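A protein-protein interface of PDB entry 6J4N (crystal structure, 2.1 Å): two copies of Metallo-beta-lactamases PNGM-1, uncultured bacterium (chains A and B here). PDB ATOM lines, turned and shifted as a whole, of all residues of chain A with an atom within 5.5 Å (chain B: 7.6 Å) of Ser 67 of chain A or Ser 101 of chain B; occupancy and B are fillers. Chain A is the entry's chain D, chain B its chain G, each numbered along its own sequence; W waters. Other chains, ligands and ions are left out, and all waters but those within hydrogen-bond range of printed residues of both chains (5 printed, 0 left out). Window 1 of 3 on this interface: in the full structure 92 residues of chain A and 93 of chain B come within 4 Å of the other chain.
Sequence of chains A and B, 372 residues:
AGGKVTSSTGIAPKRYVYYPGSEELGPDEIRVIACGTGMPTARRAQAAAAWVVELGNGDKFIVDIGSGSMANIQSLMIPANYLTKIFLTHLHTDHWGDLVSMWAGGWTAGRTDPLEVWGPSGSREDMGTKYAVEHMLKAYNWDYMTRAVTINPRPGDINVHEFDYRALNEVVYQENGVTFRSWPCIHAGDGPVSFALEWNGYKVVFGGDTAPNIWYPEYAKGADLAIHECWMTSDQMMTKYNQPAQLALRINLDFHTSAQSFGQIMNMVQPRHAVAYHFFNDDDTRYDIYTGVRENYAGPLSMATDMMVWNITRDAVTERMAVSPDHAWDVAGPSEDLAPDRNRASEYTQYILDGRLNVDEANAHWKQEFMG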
ATOM      1  N   PRO A  40     -20.439  11.497  -9.818  1.00  0.00           N
ATOM      2  CA  PRO A  40     -21.705  11.753 -10.499  1.00  0.00           C
ATOM      3  C   PRO A  40     -22.665  10.552 -10.424  1.00  0.00           C
ATOM      4  O   PRO A  40     -23.851  10.710 -10.656  1.00  0.00           O
ATOM      5  CB  PRO A  40     -21.326  12.119 -11.944  1.00  0.00           C
ATOM      6  CG  PRO A  40     -19.862  11.718 -12.088  1.00  0.00           C
ATOM      7  CD  PRO A  40     -19.274  11.698 -10.688  1.00  0.00           C
ATOM      8  N   ALA A  42     -24.871   8.255  -8.104  1.00  0.00           N
ATOM      9  CA  ALA A  42     -25.452   8.515  -6.763  1.00  0.00           C
ATOM     10  C   ALA A  42     -25.432   7.253  -5.914  1.00  0.00           C
ATOM     11  O   ALA A  42     -25.529   6.115  -6.441  1.00  0.00           O
ATOM     12  CB  ALA A  42     -26.839   9.092  -6.845  1.00  0.00           C
ATOM     13  N   ALA A  47     -22.866  11.340  -0.883  1.00  0.00           N
ATOM     14  CA  ALA A  47     -23.405  12.440  -1.682  1.00  0.00           C
ATOM     15  C   ALA A  47     -22.258  12.956  -2.545  1.00  0.00           C
ATOM     16  O   ALA A  47     -21.105  12.651  -2.231  1.00  0.00           O
ATOM     17  CB  ALA A  47     -23.956  13.517  -0.795  1.00  0.00           C
ATOM     18  N   ALA A  48     -22.580  13.665  -3.612  1.00  0.00           N
ATOM     19  CA  ALA A  48     -21.574  14.301  -4.477  1.00  0.00           C
ATOM     20  C   ALA A  48     -20.980  15.490  -3.708  1.00  0.00           C
ATOM     21  O   ALA A  48     -21.639  15.972  -2.715  1.00  0.00           O
ATOM     22  CB  ALA A  48     -22.230  14.751  -5.742  1.00  0.00           C
ATOM     23  N   ILE A  65     -21.818  22.063  -3.709  1.00  0.00           N
ATOM     24  CA  ILE A  65     -23.150  21.618  -3.219  1.00  0.00           C
ATOM     25  C   ILE A  65     -23.716  20.680  -4.306  1.00  0.00           C
ATOM     26  O   ILE A  65     -24.728  21.012  -4.993  1.00  0.00           O
ATOM     27  CB  ILE A  65     -23.991  22.863  -2.837  1.00  0.00           C
ATOM     28  CG1 ILE A  65     -25.308  22.473  -2.160  1.00  0.00           C
ATOM     29  CG2 ILE A  65     -24.159  23.789  -4.041  1.00  0.00           C
ATOM     30  CD1 ILE A  65     -25.997  23.586  -1.394  1.00  0.00           C
ATOM     31  N   GLY A  66     -23.058  19.522  -4.404  1.00  0.00           N
ATOM     32  CA  GLY A  66     -23.334  18.411  -5.337  1.00  0.00           C
ATOM     33  C   GLY A  66     -24.646  17.726  -5.010  1.00  0.00           C
ATOM     34  O   GLY A  66     -25.098  17.760  -3.832  1.00  0.00           O
ATOM     35  N   SER A  67     -25.257  17.115  -6.029  1.00  0.00           N
ATOM     36  CA  SER A  67     -26.463  16.267  -5.906  1.00  0.00           C
ATOM     37  C   SER A  67     -26.409  15.444  -4.621  1.00  0.00           C
ATOM     38  O   SER A  67     -25.405  14.807  -4.380  1.00  0.00           O
ATOM     39  CB  SER A  67     -26.650  15.407  -7.158  1.00  0.00           C
ATOM     40  OG  SER A  67     -26.821  16.263  -8.295  1.00  0.00           O
ATOM     41  N   GLY A  68     -27.495  15.460  -3.856  1.00  0.00           N
ATOM     42  CA  GLY A  68     -27.660  14.697  -2.605  1.00  0.00           C
ATOM     43  C   GLY A  68     -27.052  15.349  -1.362  1.00  0.00           C
ATOM     44  O   GLY A  68     -27.423  14.942  -0.229  1.00  0.00           O
ATOM     45  N   SER A  69     -26.175  16.342  -1.499  1.00  0.00           N
ATOM     46  CA  SER A  69     -25.389  16.860  -0.344  1.00  0.00           C
ATOM     47  C   SER A  69     -26.312  17.612   0.651  1.00  0.00           C
ATOM     48  O   SER A  69     -26.039  17.615   1.859  1.00  0.00           O
ATOM     49  CB  SER A  69     -24.242  17.713  -0.839  1.00  0.00           C
ATOM     50  OG  SER A  69     -24.746  18.921  -1.375  1.00  0.00           O
ATOM     51  N   THR A  93     -22.611  18.588 -12.470  1.00  0.00           N
ATOM     52  CA  THR A  93     -23.802  18.362 -11.614  1.00  0.00           C
ATOM     53  C   THR A  93     -23.396  17.882 -10.231  1.00  0.00           C
ATOM     54  O   THR A  93     -24.091  18.211  -9.258  1.00  0.00           O
ATOM     55  CB  THR A  93     -24.813  17.395 -12.221  1.00  0.00           C
ATOM     56  OG1 THR A  93     -24.213  16.098 -12.246  1.00  0.00           O
ATOM     57  CG2 THR A  93     -25.262  17.875 -13.577  1.00  0.00           C
ATOM     58  N   ASP A  94     -22.307  17.151 -10.111  1.00  0.00           N
ATOM     59  CA  ASP A  94     -21.926  16.638  -8.773  1.00  0.00           C
ATOM     60  C   ASP A  94     -21.216  17.726  -7.937  1.00  0.00           C
ATOM     61  O   ASP A  94     -20.671  17.404  -6.819  1.00  0.00           O
ATOM     62  CB  ASP A  94     -21.186  15.312  -8.907  1.00  0.00           C
ATOM     63  CG  ASP A  94     -19.922  15.426  -9.704  1.00  0.00           C
ATOM     64  OD1 ASP A  94     -18.862  15.029  -9.187  1.00  0.00           O
ATOM     65  OD2 ASP A  94     -20.021  15.916 -10.820  1.00  0.00           O
ATOM     66  N   HIS A  95     -21.230  18.971  -8.398  1.00  0.00           N
ATOM     67  CA  HIS A  95     -20.633  20.086  -7.623  1.00  0.00           C
ATOM     68  C   HIS A  95     -21.625  21.217  -7.399  1.00  0.00           C
ATOM     69  O   HIS A  95     -21.292  22.033  -6.546  1.00  0.00           O
ATOM     70  CB  HIS A  95     -19.337  20.585  -8.277  1.00  0.00           C
ATOM     71  CG  HIS A  95     -18.245  19.592  -8.147  1.00  0.00           C
ATOM     72  ND1 HIS A  95     -17.264  19.706  -7.174  1.00  0.00           N
ATOM     73  CD2 HIS A  95     -18.039  18.406  -8.774  1.00  0.00           C
ATOM     74  CE1 HIS A  95     -16.483  18.649  -7.235  1.00  0.00           C
ATOM     75  NE2 HIS A  95     -16.933  17.827  -8.206  1.00  0.00           N
ATOM     76  N   TRP A  96     -22.730  21.327  -8.161  1.00  0.00           N
ATOM     77  CA  TRP A  96     -23.757  22.371  -7.865  1.00  0.00           C
ATOM     78  C   TRP A  96     -25.219  21.909  -8.058  1.00  0.00           C
ATOM     79  O   TRP A  96     -26.133  22.772  -7.973  1.00  0.00           O
ATOM     80  CB  TRP A  96     -23.406  23.653  -8.627  1.00  0.00           C
ATOM     81  CG  TRP A  96     -23.734  23.649 -10.078  1.00  0.00           C
ATOM     82  CD1 TRP A  96     -23.138  22.931 -11.079  1.00  0.00           C
ATOM     83  CD2 TRP A  96     -24.728  24.467 -10.694  1.00  0.00           C
ATOM     84  NE1 TRP A  96     -23.714  23.243 -12.282  1.00  0.00           N
ATOM     85  CE2 TRP A  96     -24.709  24.161 -12.069  1.00  0.00           C
ATOM     86  CE3 TRP A  96     -25.633  25.416 -10.217  1.00  0.00           C
ATOM     87  CZ2 TRP A  96     -25.567  24.780 -12.965  1.00  0.00           C
ATOM     88  CZ3 TRP A  96     -26.509  25.999 -11.102  1.00  0.00           C
ATOM     89  CH2 TRP A  96     -26.462  25.689 -12.461  1.00  0.00           C
ATOM     90  N   GLY A  97     -25.431  20.590  -8.229  1.00  0.00           N
ATOM     91  CA  GLY A  97     -26.739  19.925  -8.363  1.00  0.00           C
ATOM     92  C   GLY A  97     -27.696  20.308  -7.243  1.00  0.00           C
ATOM     93  O   GLY A  97     -28.879  20.566  -7.571  1.00  0.00           O
ATOM     94  N   ASP A  98     -27.220  20.498  -6.000  1.00  0.00           N
ATOM     95  CA  ASP A  98     -28.127  20.778  -4.848  1.00  0.00           C
ATOM     96  C   ASP A  98     -28.229  22.271  -4.543  1.00  0.00           C
ATOM     97  O   ASP A  98     -28.886  22.654  -3.534  1.00  0.00           O
ATOM     98  CB  ASP A  98     -27.752  19.979  -3.590  1.00  0.00           C
ATOM     99  CG  ASP A  98     -28.572  18.687  -3.477  1.00  0.00           C
ATOM    100  OD1 ASP A  98     -29.228  18.353  -4.492  1.00  0.00           O
ATOM    101  OD2 ASP A  98     -28.646  18.062  -2.384  1.00  0.00           O
ATOM    102  N   ILE B  65     -38.938  12.672  -9.734  1.00  0.00           N
ATOM    103  CA  ILE B  65     -37.479  12.433  -9.540  1.00  0.00           C
ATOM    104  C   ILE B  65     -36.890  13.626  -8.762  1.00  0.00           C
ATOM    105  O   ILE B  65     -36.064  14.433  -9.260  1.00  0.00           O
ATOM    106  CB  ILE B  65     -36.814  12.149 -10.887  1.00  0.00           C
ATOM    107  CG1 ILE B  65     -35.382  11.669 -10.635  1.00  0.00           C
ATOM    108  CG2 ILE B  65     -36.930  13.337 -11.832  1.00  0.00           C
ATOM    109  CD1 ILE B  65     -34.652  11.148 -11.850  1.00  0.00           C
ATOM    110  N   SER B  67     -35.126  15.816  -5.604  1.00  0.00           N
ATOM    111  CA  SER B  67     -33.768  15.983  -5.022  1.00  0.00           C
ATOM    112  C   SER B  67     -33.418  14.783  -4.137  1.00  0.00           C
ATOM    113  O   SER B  67     -34.228  14.393  -3.305  1.00  0.00           O
ATOM    114  CB  SER B  67     -33.739  17.297  -4.236  1.00  0.00           C
ATOM    115  OG  SER B  67     -34.202  18.392  -5.030  1.00  0.00           O
ATOM    116  N   GLY B  68     -32.254  14.189  -4.335  1.00  0.00           N
ATOM    117  CA  GLY B  68     -31.795  13.081  -3.507  1.00  0.00           C
ATOM    118  C   GLY B  68     -32.268  11.732  -4.020  1.00  0.00           C
ATOM    119  O   GLY B  68     -31.642  10.758  -3.656  1.00  0.00           O
ATOM    120  N   SER B  69     -33.360  11.637  -4.791  1.00  0.00           N
ATOM    121  CA  SER B  69     -33.960  10.319  -5.143  1.00  0.00           C
ATOM    122  C   SER B  69     -32.992   9.447  -5.950  1.00  0.00           C
ATOM    123  O   SER B  69     -33.118   8.206  -5.866  1.00  0.00           O
ATOM    124  CB  SER B  69     -35.312  10.444  -5.854  1.00  0.00           C
ATOM    125  OG  SER B  69     -35.205  11.165  -7.075  1.00  0.00           O
ATOM    126  N   MET B  70     -32.011  10.011  -6.660  1.00  0.00           N
ATOM    127  CA  MET B  70     -31.165   9.179  -7.565  1.00  0.00           C
ATOM    128  C   MET B  70     -30.374   8.146  -6.770  1.00  0.00           C
ATOM    129  O   MET B  70     -29.985   7.081  -7.329  1.00  0.00           O
ATOM    130  CB  MET B  70     -30.165  10.038  -8.343  1.00  0.00           C
ATOM    131  CG  MET B  70     -29.649   9.343  -9.593  1.00  0.00           C
ATOM    132  SD  MET B  70     -30.984   8.951 -10.806  1.00  0.00           S
ATOM    133  CE  MET B  70     -29.997   7.681 -11.591  1.00  0.00           C
ATOM    134  N   ALA B  71     -30.061   8.442  -5.508  1.00  0.00           N
ATOM    135  CA  ALA B  71     -29.290   7.488  -4.678  1.00  0.00           C
ATOM    136  C   ALA B  71     -30.126   6.216  -4.503  1.00  0.00           C
ATOM    137  O   ALA B  71     -29.589   5.096  -4.524  1.00  0.00           O
ATOM    138  CB  ALA B  71     -28.930   8.089  -3.337  1.00  0.00           C
ATOM    139  N   GLN B  74     -30.607   4.381  -7.946  1.00  0.00           N
ATOM    140  CA  GLN B  74     -29.362   3.719  -8.380  1.00  0.00           C
ATOM    141  C   GLN B  74     -29.125   2.466  -7.555  1.00  0.00           C
ATOM    142  O   GLN B  74     -28.324   1.631  -7.995  1.00  0.00           O
ATOM    143  CB  GLN B  74     -28.200   4.679  -8.194  1.00  0.00           C
ATOM    144  CG  GLN B  74     -26.867   4.185  -8.708  1.00  0.00           C
ATOM    145  CD  GLN B  74     -26.973   3.902 -10.191  1.00  0.00           C
ATOM    146  OE1 GLN B  74     -26.906   4.818 -11.014  1.00  0.00           O
ATOM    147  NE2 GLN B  74     -27.229   2.641 -10.531  1.00  0.00           N
ATOM    148  N   TRP B  96     -38.636  17.125  -9.316  1.00  0.00           N
ATOM    149  CA  TRP B  96     -37.774  16.929 -10.532  1.00  0.00           C
ATOM    150  C   TRP B  96     -36.329  17.466 -10.380  1.00  0.00           C
ATOM    151  O   TRP B  96     -35.549  17.477 -11.381  1.00  0.00           O
ATOM    152  CB  TRP B  96     -38.465  17.515 -11.788  1.00  0.00           C
ATOM    153  CG  TRP B  96     -38.473  19.011 -11.920  1.00  0.00           C
ATOM    154  CD1 TRP B  96     -39.109  19.933 -11.140  1.00  0.00           C
ATOM    155  CD2 TRP B  96     -37.761  19.774 -12.906  1.00  0.00           C
ATOM    156  NE1 TRP B  96     -38.886  21.212 -11.608  1.00  0.00           N
ATOM    157  CE2 TRP B  96     -38.033  21.138 -12.677  1.00  0.00           C
ATOM    158  CE3 TRP B  96     -36.929  19.424 -13.963  1.00  0.00           C
ATOM    159  CZ2 TRP B  96     -37.514  22.143 -13.486  1.00  0.00           C
ATOM    160  CZ3 TRP B  96     -36.412  20.421 -14.749  1.00  0.00           C
ATOM    161  CH2 TRP B  96     -36.697  21.756 -14.516  1.00  0.00           C
ATOM    162  N   GLY B  97     -35.937  17.845  -9.170  1.00  0.00           N
ATOM    163  CA  GLY B  97     -34.547  18.225  -8.821  1.00  0.00           C
ATOM    164  C   GLY B  97     -33.470  17.240  -9.257  1.00  0.00           C
ATOM    165  O   GLY B  97     -32.410  17.691  -9.644  1.00  0.00           O
ATOM    166  N   ASP B  98     -33.693  15.935  -9.202  1.00  0.00           N
ATOM    167  CA  ASP B  98     -32.686  14.941  -9.652  1.00  0.00           C
ATOM    168  C   ASP B  98     -32.843  14.586 -11.144  1.00  0.00           C
ATOM    169  O   ASP B  98     -32.115  13.720 -11.595  1.00  0.00           O
ATOM    170  CB  ASP B  98     -32.713  13.685  -8.767  1.00  0.00           C
ATOM    171  CG  ASP B  98     -31.742  13.776  -7.608  1.00  0.00           C
ATOM    172  OD1 ASP B  98     -31.341  14.930  -7.306  1.00  0.00           O
ATOM    173  OD2 ASP B  98     -31.377  12.714  -7.008  1.00  0.00           O
ATOM    174  N   LEU B  99     -33.690  15.260 -11.916  1.00  0.00           N
ATOM    175  CA  LEU B  99     -33.715  15.000 -13.374  1.00  0.00           C
ATOM    176  C   LEU B  99     -32.290  15.230 -13.866  1.00  0.00           C
ATOM    177  O   LEU B  99     -31.767  14.371 -14.573  1.00  0.00           O
ATOM    178  CB  LEU B  99     -34.709  15.907 -14.119  1.00  0.00           C
ATOM    179  CG  LEU B  99     -34.647  15.769 -15.647  1.00  0.00           C
ATOM    180  CD1 LEU B  99     -35.064  14.362 -16.033  1.00  0.00           C
ATOM    181  CD2 LEU B  99     -35.495  16.804 -16.355  1.00  0.00           C
ATOM    182  N   VAL B 100     -31.645  16.335 -13.455  1.00  0.00           N
ATOM    183  CA  VAL B 100     -30.301  16.678 -14.022  1.00  0.00           C
ATOM    184  C   VAL B 100     -29.321  15.541 -13.754  1.00  0.00           C
ATOM    185  O   VAL B 100     -28.468  15.255 -14.610  1.00  0.00           O
ATOM    186  CB  VAL B 100     -29.722  17.995 -13.491  1.00  0.00           C
ATOM    187  CG1 VAL B 100     -29.460  17.918 -12.004  1.00  0.00           C
ATOM    188  CG2 VAL B 100     -28.453  18.361 -14.266  1.00  0.00           C
ATOM    189  N   SER B 101     -29.453  14.930 -12.589  1.00  0.00           N
ATOM    190  CA  SER B 101     -28.546  13.863 -12.117  1.00  0.00           C
ATOM    191  C   SER B 101     -28.767  12.541 -12.878  1.00  0.00           C
ATOM    192  O   SER B 101     -27.775  11.873 -13.176  1.00  0.00           O
ATOM    193  CB  SER B 101     -28.712  13.771 -10.637  1.00  0.00           C
ATOM    194  OG  SER B 101     -28.210  12.560 -10.146  1.00  0.00           O
ATOM    195  N   MET B 102     -30.012  12.192 -13.228  1.00  0.00           N
ATOM    196  CA  MET B 102     -30.299  11.043 -14.129  1.00  0.00           C
ATOM    197  C   MET B 102     -29.822  11.384 -15.537  1.00  0.00           C
ATOM    198  O   MET B 102     -29.404  10.464 -16.285  1.00  0.00           O
ATOM    199  CB  MET B 102     -31.805  10.785 -14.191  1.00  0.00           C
ATOM    200  CG  MET B 102     -32.249   9.881 -15.313  1.00  0.00           C
ATOM    201  SD  MET B 102     -31.783   8.206 -14.940  1.00  0.00           S
ATOM    202  CE  MET B 102     -33.301   7.751 -14.105  1.00  0.00           C
ATOM    203  N   TRP B 103     -30.004  12.645 -15.923  1.00  0.00           N
ATOM    204  CA  TRP B 103     -29.602  13.121 -17.266  1.00  0.00           C
ATOM    205  C   TRP B 103     -28.089  12.959 -17.446  1.00  0.00           C
ATOM    206  O   TRP B 103     -27.699  12.308 -18.408  1.00  0.00           O
ATOM    207  CB  TRP B 103     -30.057  14.560 -17.453  1.00  0.00           C
ATOM    208  CG  TRP B 103     -29.432  15.262 -18.607  1.00  0.00           C
ATOM    209  CD1 TRP B 103     -29.692  15.075 -19.931  1.00  0.00           C
ATOM    210  CD2 TRP B 103     -28.469  16.320 -18.526  1.00  0.00           C
ATOM    211  NE1 TRP B 103     -28.945  15.939 -20.679  1.00  0.00           N
ATOM    212  CE2 TRP B 103     -28.182  16.712 -19.847  1.00  0.00           C
ATOM    213  CE3 TRP B 103     -27.804  16.950 -17.468  1.00  0.00           C
ATOM    214  CZ2 TRP B 103     -27.283  17.739 -20.137  1.00  0.00           C
ATOM    215  CZ3 TRP B 103     -26.934  17.979 -17.750  1.00  0.00           C
ATOM    216  CH2 TRP B 103     -26.667  18.355 -19.071  1.00  0.00           C
ATOM    217  N   ALA B 104     -27.290  13.486 -16.517  1.00  0.00           N
ATOM    218  CA  ALA B 104     -25.814  13.545 -16.616  1.00  0.00           C
ATOM    219  C   ALA B 104     -25.179  12.224 -16.177  1.00  0.00           C
ATOM    220  O   ALA B 104     -24.300  11.761 -16.863  1.00  0.00           O
ATOM    221  CB  ALA B 104     -25.277  14.669 -15.766  1.00  0.00           C
ATOM    222  N   GLY B 105     -25.592  11.662 -15.044  1.00  0.00           N
ATOM    223  CA  GLY B 105     -25.059  10.380 -14.557  1.00  0.00           C
ATOM    224  C   GLY B 105     -25.374   9.231 -15.510  1.00  0.00           C
ATOM    225  O   GLY B 105     -24.480   8.416 -15.761  1.00  0.00           O
ATOM    226  N   GLY B 106     -26.590   9.173 -16.051  1.00  0.00           N
ATOM    227  CA  GLY B 106     -27.004   8.064 -16.928  1.00  0.00           C
ATOM    228  C   GLY B 106     -26.261   8.126 -18.249  1.00  0.00           C
ATOM    229  O   GLY B 106     -26.073   7.068 -18.895  1.00  0.00           O
ATOM    230  N   TRP B 107     -25.843   9.324 -18.643  1.00  0.00           N
ATOM    231  CA  TRP B 107     -25.064   9.559 -19.882  1.00  0.00           C
ATOM    232  C   TRP B 107     -23.574   9.273 -19.608  1.00  0.00           C
ATOM    233  O   TRP B 107     -22.960   8.592 -20.424  1.00  0.00           O
ATOM    234  CB  TRP B 107     -25.406  10.974 -20.372  1.00  0.00           C
ATOM    235  CG  TRP B 107     -24.728  11.487 -21.602  1.00  0.00           C
ATOM    236  CD1 TRP B 107     -24.154  10.790 -22.625  1.00  0.00           C
ATOM    237  CD2 TRP B 107     -24.607  12.874 -21.952  1.00  0.00           C
ATOM    238  NE1 TRP B 107     -23.664  11.653 -23.572  1.00  0.00           N
ATOM    239  CE2 TRP B 107     -23.931  12.933 -23.185  1.00  0.00           C
ATOM    240  CE3 TRP B 107     -24.986  14.065 -21.327  1.00  0.00           C
ATOM    241  CZ2 TRP B 107     -23.635  14.139 -23.803  1.00  0.00           C
ATOM    242  CZ3 TRP B 107     -24.697  15.254 -21.944  1.00  0.00           C
ATOM    243  CH2 TRP B 107     -24.019  15.287 -23.155  1.00  0.00           C
ATOM    244  N   THR B 108     -23.010   9.699 -18.473  1.00  0.00           N
ATOM    245  CA  THR B 108     -21.628   9.308 -18.077  1.00  0.00           C
ATOM    246  C   THR B 108     -21.571   7.783 -17.924  1.00  0.00           C
ATOM    247  O   THR B 108     -20.463   7.206 -18.096  1.00  0.00           O
ATOM    248  CB  THR B 108     -21.131   9.978 -16.785  1.00  0.00           C
ATOM    249  OG1 THR B 108     -21.805   9.431 -15.650  1.00  0.00           O
ATOM    250  CG2 THR B 108     -21.282  11.483 -16.795  1.00  0.00           C
ATOM    251  N   ARG B 111     -26.117   5.418 -20.806  1.00  0.00           N
ATOM    252  CA  ARG B 111     -27.431   5.493 -21.490  1.00  0.00           C
ATOM    253  C   ARG B 111     -27.091   5.889 -22.914  1.00  0.00           C
ATOM    254  O   ARG B 111     -26.310   6.854 -23.100  1.00  0.00           O
ATOM    255  CB  ARG B 111     -28.431   6.510 -20.923  1.00  0.00           C
ATOM    256  CG  ARG B 111     -29.577   6.820 -21.878  1.00  0.00           C
ATOM    257  CD  ARG B 111     -30.525   7.913 -21.428  1.00  0.00           C
ATOM    258  NE  ARG B 111     -29.934   9.252 -21.469  1.00  0.00           N
ATOM    259  CZ  ARG B 111     -29.554   9.959 -20.397  1.00  0.00           C
ATOM    260  NH1 ARG B 111     -29.700   9.479 -19.174  1.00  0.00           N
ATOM    261  NH2 ARG B 111     -29.026  11.163 -20.548  1.00  0.00           N
ATOM    262  N   LEU B 115     -33.251  11.165 -22.920  1.00  0.00           N
ATOM    263  CA  LEU B 115     -34.322  11.006 -21.912  1.00  0.00           C
ATOM    264  C   LEU B 115     -35.603  11.496 -22.552  1.00  0.00           C
ATOM    265  O   LEU B 115     -35.577  12.387 -23.441  1.00  0.00           O
ATOM    266  CB  LEU B 115     -34.089  11.775 -20.613  1.00  0.00           C
ATOM    267  CG  LEU B 115     -33.002  11.230 -19.703  1.00  0.00           C
ATOM    268  CD1 LEU B 115     -32.874  12.156 -18.505  1.00  0.00           C
ATOM    269  CD2 LEU B 115     -33.276   9.795 -19.248  1.00  0.00           C
ATOM    270  N   MET B 136     -33.219  24.177 -18.042  1.00  0.00           N
ATOM    271  CA  MET B 136     -32.349  23.278 -17.244  1.00  0.00           C
ATOM    272  C   MET B 136     -31.158  22.879 -18.112  1.00  0.00           C
ATOM    273  O   MET B 136     -30.029  22.902 -17.623  1.00  0.00           O
ATOM    274  CB  MET B 136     -33.095  22.015 -16.824  1.00  0.00           C
ATOM    275  CG  MET B 136     -32.320  21.125 -15.892  1.00  0.00           C
ATOM    276  SD  MET B 136     -32.753  19.364 -16.136  1.00  0.00           S
ATOM    277  CE  MET B 136     -31.624  18.996 -17.465  1.00  0.00           C
ATOM    278  N   TYR B 140     -27.214  23.837 -17.329  1.00  0.00           N
ATOM    279  CA  TYR B 140     -26.120  22.848 -17.332  1.00  0.00           C
ATOM    280  C   TYR B 140     -25.349  22.832 -18.661  1.00  0.00           C
ATOM    281  O   TYR B 140     -24.707  21.807 -18.973  1.00  0.00           O
ATOM    282  CB  TYR B 140     -26.668  21.502 -16.889  1.00  0.00           C
ATOM    283  CG  TYR B 140     -27.059  21.508 -15.436  1.00  0.00           C
ATOM    284  CD1 TYR B 140     -26.120  21.364 -14.432  1.00  0.00           C
ATOM    285  CD2 TYR B 140     -28.365  21.734 -15.060  1.00  0.00           C
ATOM    286  CE1 TYR B 140     -26.479  21.421 -13.089  1.00  0.00           C
ATOM    287  CE2 TYR B 140     -28.744  21.768 -13.725  1.00  0.00           C
ATOM    288  CZ  TYR B 140     -27.798  21.621 -12.731  1.00  0.00           C
ATOM    289  OH  TYR B 140     -28.217  21.625 -11.424  1.00  0.00           O
HETATM  290  O   HOH W   1     -28.681  23.328  -8.978  1.00  0.00           O
HETATM  291  O   HOH W   2     -26.507   7.155  -9.914  1.00  0.00           O
HETATM  292  O   HOH W   3     -30.224  16.153  -5.364  1.00  0.00           O
HETATM  293  O   HOH W   4     -29.322  16.666  -8.603  1.00  0.00           O
HETATM  294  O   HOH W   5     -31.632  18.963  -5.956  1.00  0.00           O
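Water W3 lies within hydrogen-bond range of OD1 of Asp 98 of chain B (2.6 Å), OD1 of Asp 98 of chain A (2.6 Å), N of Gly 68 of chain B (3.0 Å) and N of Gly 68 of chain A (3.2 Å).
Water W4 lies within hydrogen-bond range of the side-chain hydroxyl of Ser 67 of chain A (2.6 Å), the side-chain carboxylate of Asp 98 of chain B (3.0 Å) and the backbone carbonyl oxygen of Gly 97 of chain B (3.4 Å).
Water W2 lies within hydrogen-bond range of OE1 of Gln 74 of chain B (2.6 Å) and N of Ala 42 of chain A (2.7 Å).
Water W5 bridges the side-chain hydroxyl of Ser 67 of chain B (2.8 Å) and the side-chain carboxylate of Asp 98 of chain A (2.9 Å).
Water W1 lies within hydrogen-bond range of the backbone carbonyl oxygen of Trp 96 of chain A (2.8 Å), the side-chain hydroxyl of Tyr 140 of chain B (3.0 Å) and the backbone carbonyl oxygen of Gly 97 of chain A (3.1 Å).
Printed residues of chain B within 4 Å of Ser 67 of chain A: Ser 101.
Ser 101 of chain B touches just one residue of chain A: Ser 67.
Of the printed residues of chain A, Met 70 of chain B touches Ala 42 (3.7 Å).
Of the printed residues of chain B, Ala 42 of chain A touches Met 70, Ala 71 and Gln 74.
Of the printed residues of chain A, Ala 71 of chain B touches Ala 42 (3.5 Å).
Asp 98 of chain B touches none of the printed residues of chain A.
The backbone NH (N) of Ala 48 of chain A sits at hydrogen-bond distance from the backbone carbonyl oxygen (O) of Ser 67 of chain A (3.1 Å).
The backbone NH (N) of Gly 97 of chain A is in hydrogen-bond range of the backbone carbonyl oxygen (O) of Ile 65 of chain A (3.3 Å).
OG of Ser 67 of chain A is in hydrogen-bond range of O of Thr 93 of chain A (3.5 Å).
The backbone NH (N) of Met 70 of chain B is in hydrogen-bond range of the side-chain carboxylate (OD2) of Asp 98 of chain B (2.8 Å).
7 positions are printed for both chains.
Of the 15 printed residues of chain A, 5 touch a printed residue of chain B.
Hydrophobic or aromatic side chains of chain B that line the printed part of chain A: Met 70, Val 100, Ala 104 and Tyr 140.
Ala 42 of chain A touches Met 70 of chain B (CB to C, 3.7 Å).
Ala 71 of chain B touches Ala 42 of chain A (N to CB, 3.5 Å).
Ala 42 of chain A touches Gln 74 of chain B.
CB of Ser 101 of chain B touches OG of Ser 67 of chain A (3.9 Å).
Val 100 of chain B touches Thr 93 of chain A (CG2 to CG2, 3.3 Å).
CG2 of Thr 93 of chain A touches CB of Ala 104 of chain B, at 3.9 Å.
Thr 93 of chain A touches Tyr 140 of chain B.
Trp 96 of chain A touches Tyr 140 of chain B.
Gly 97 of chain A touches Tyr 140 of chain B (CA to OH, 3.8 Å).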
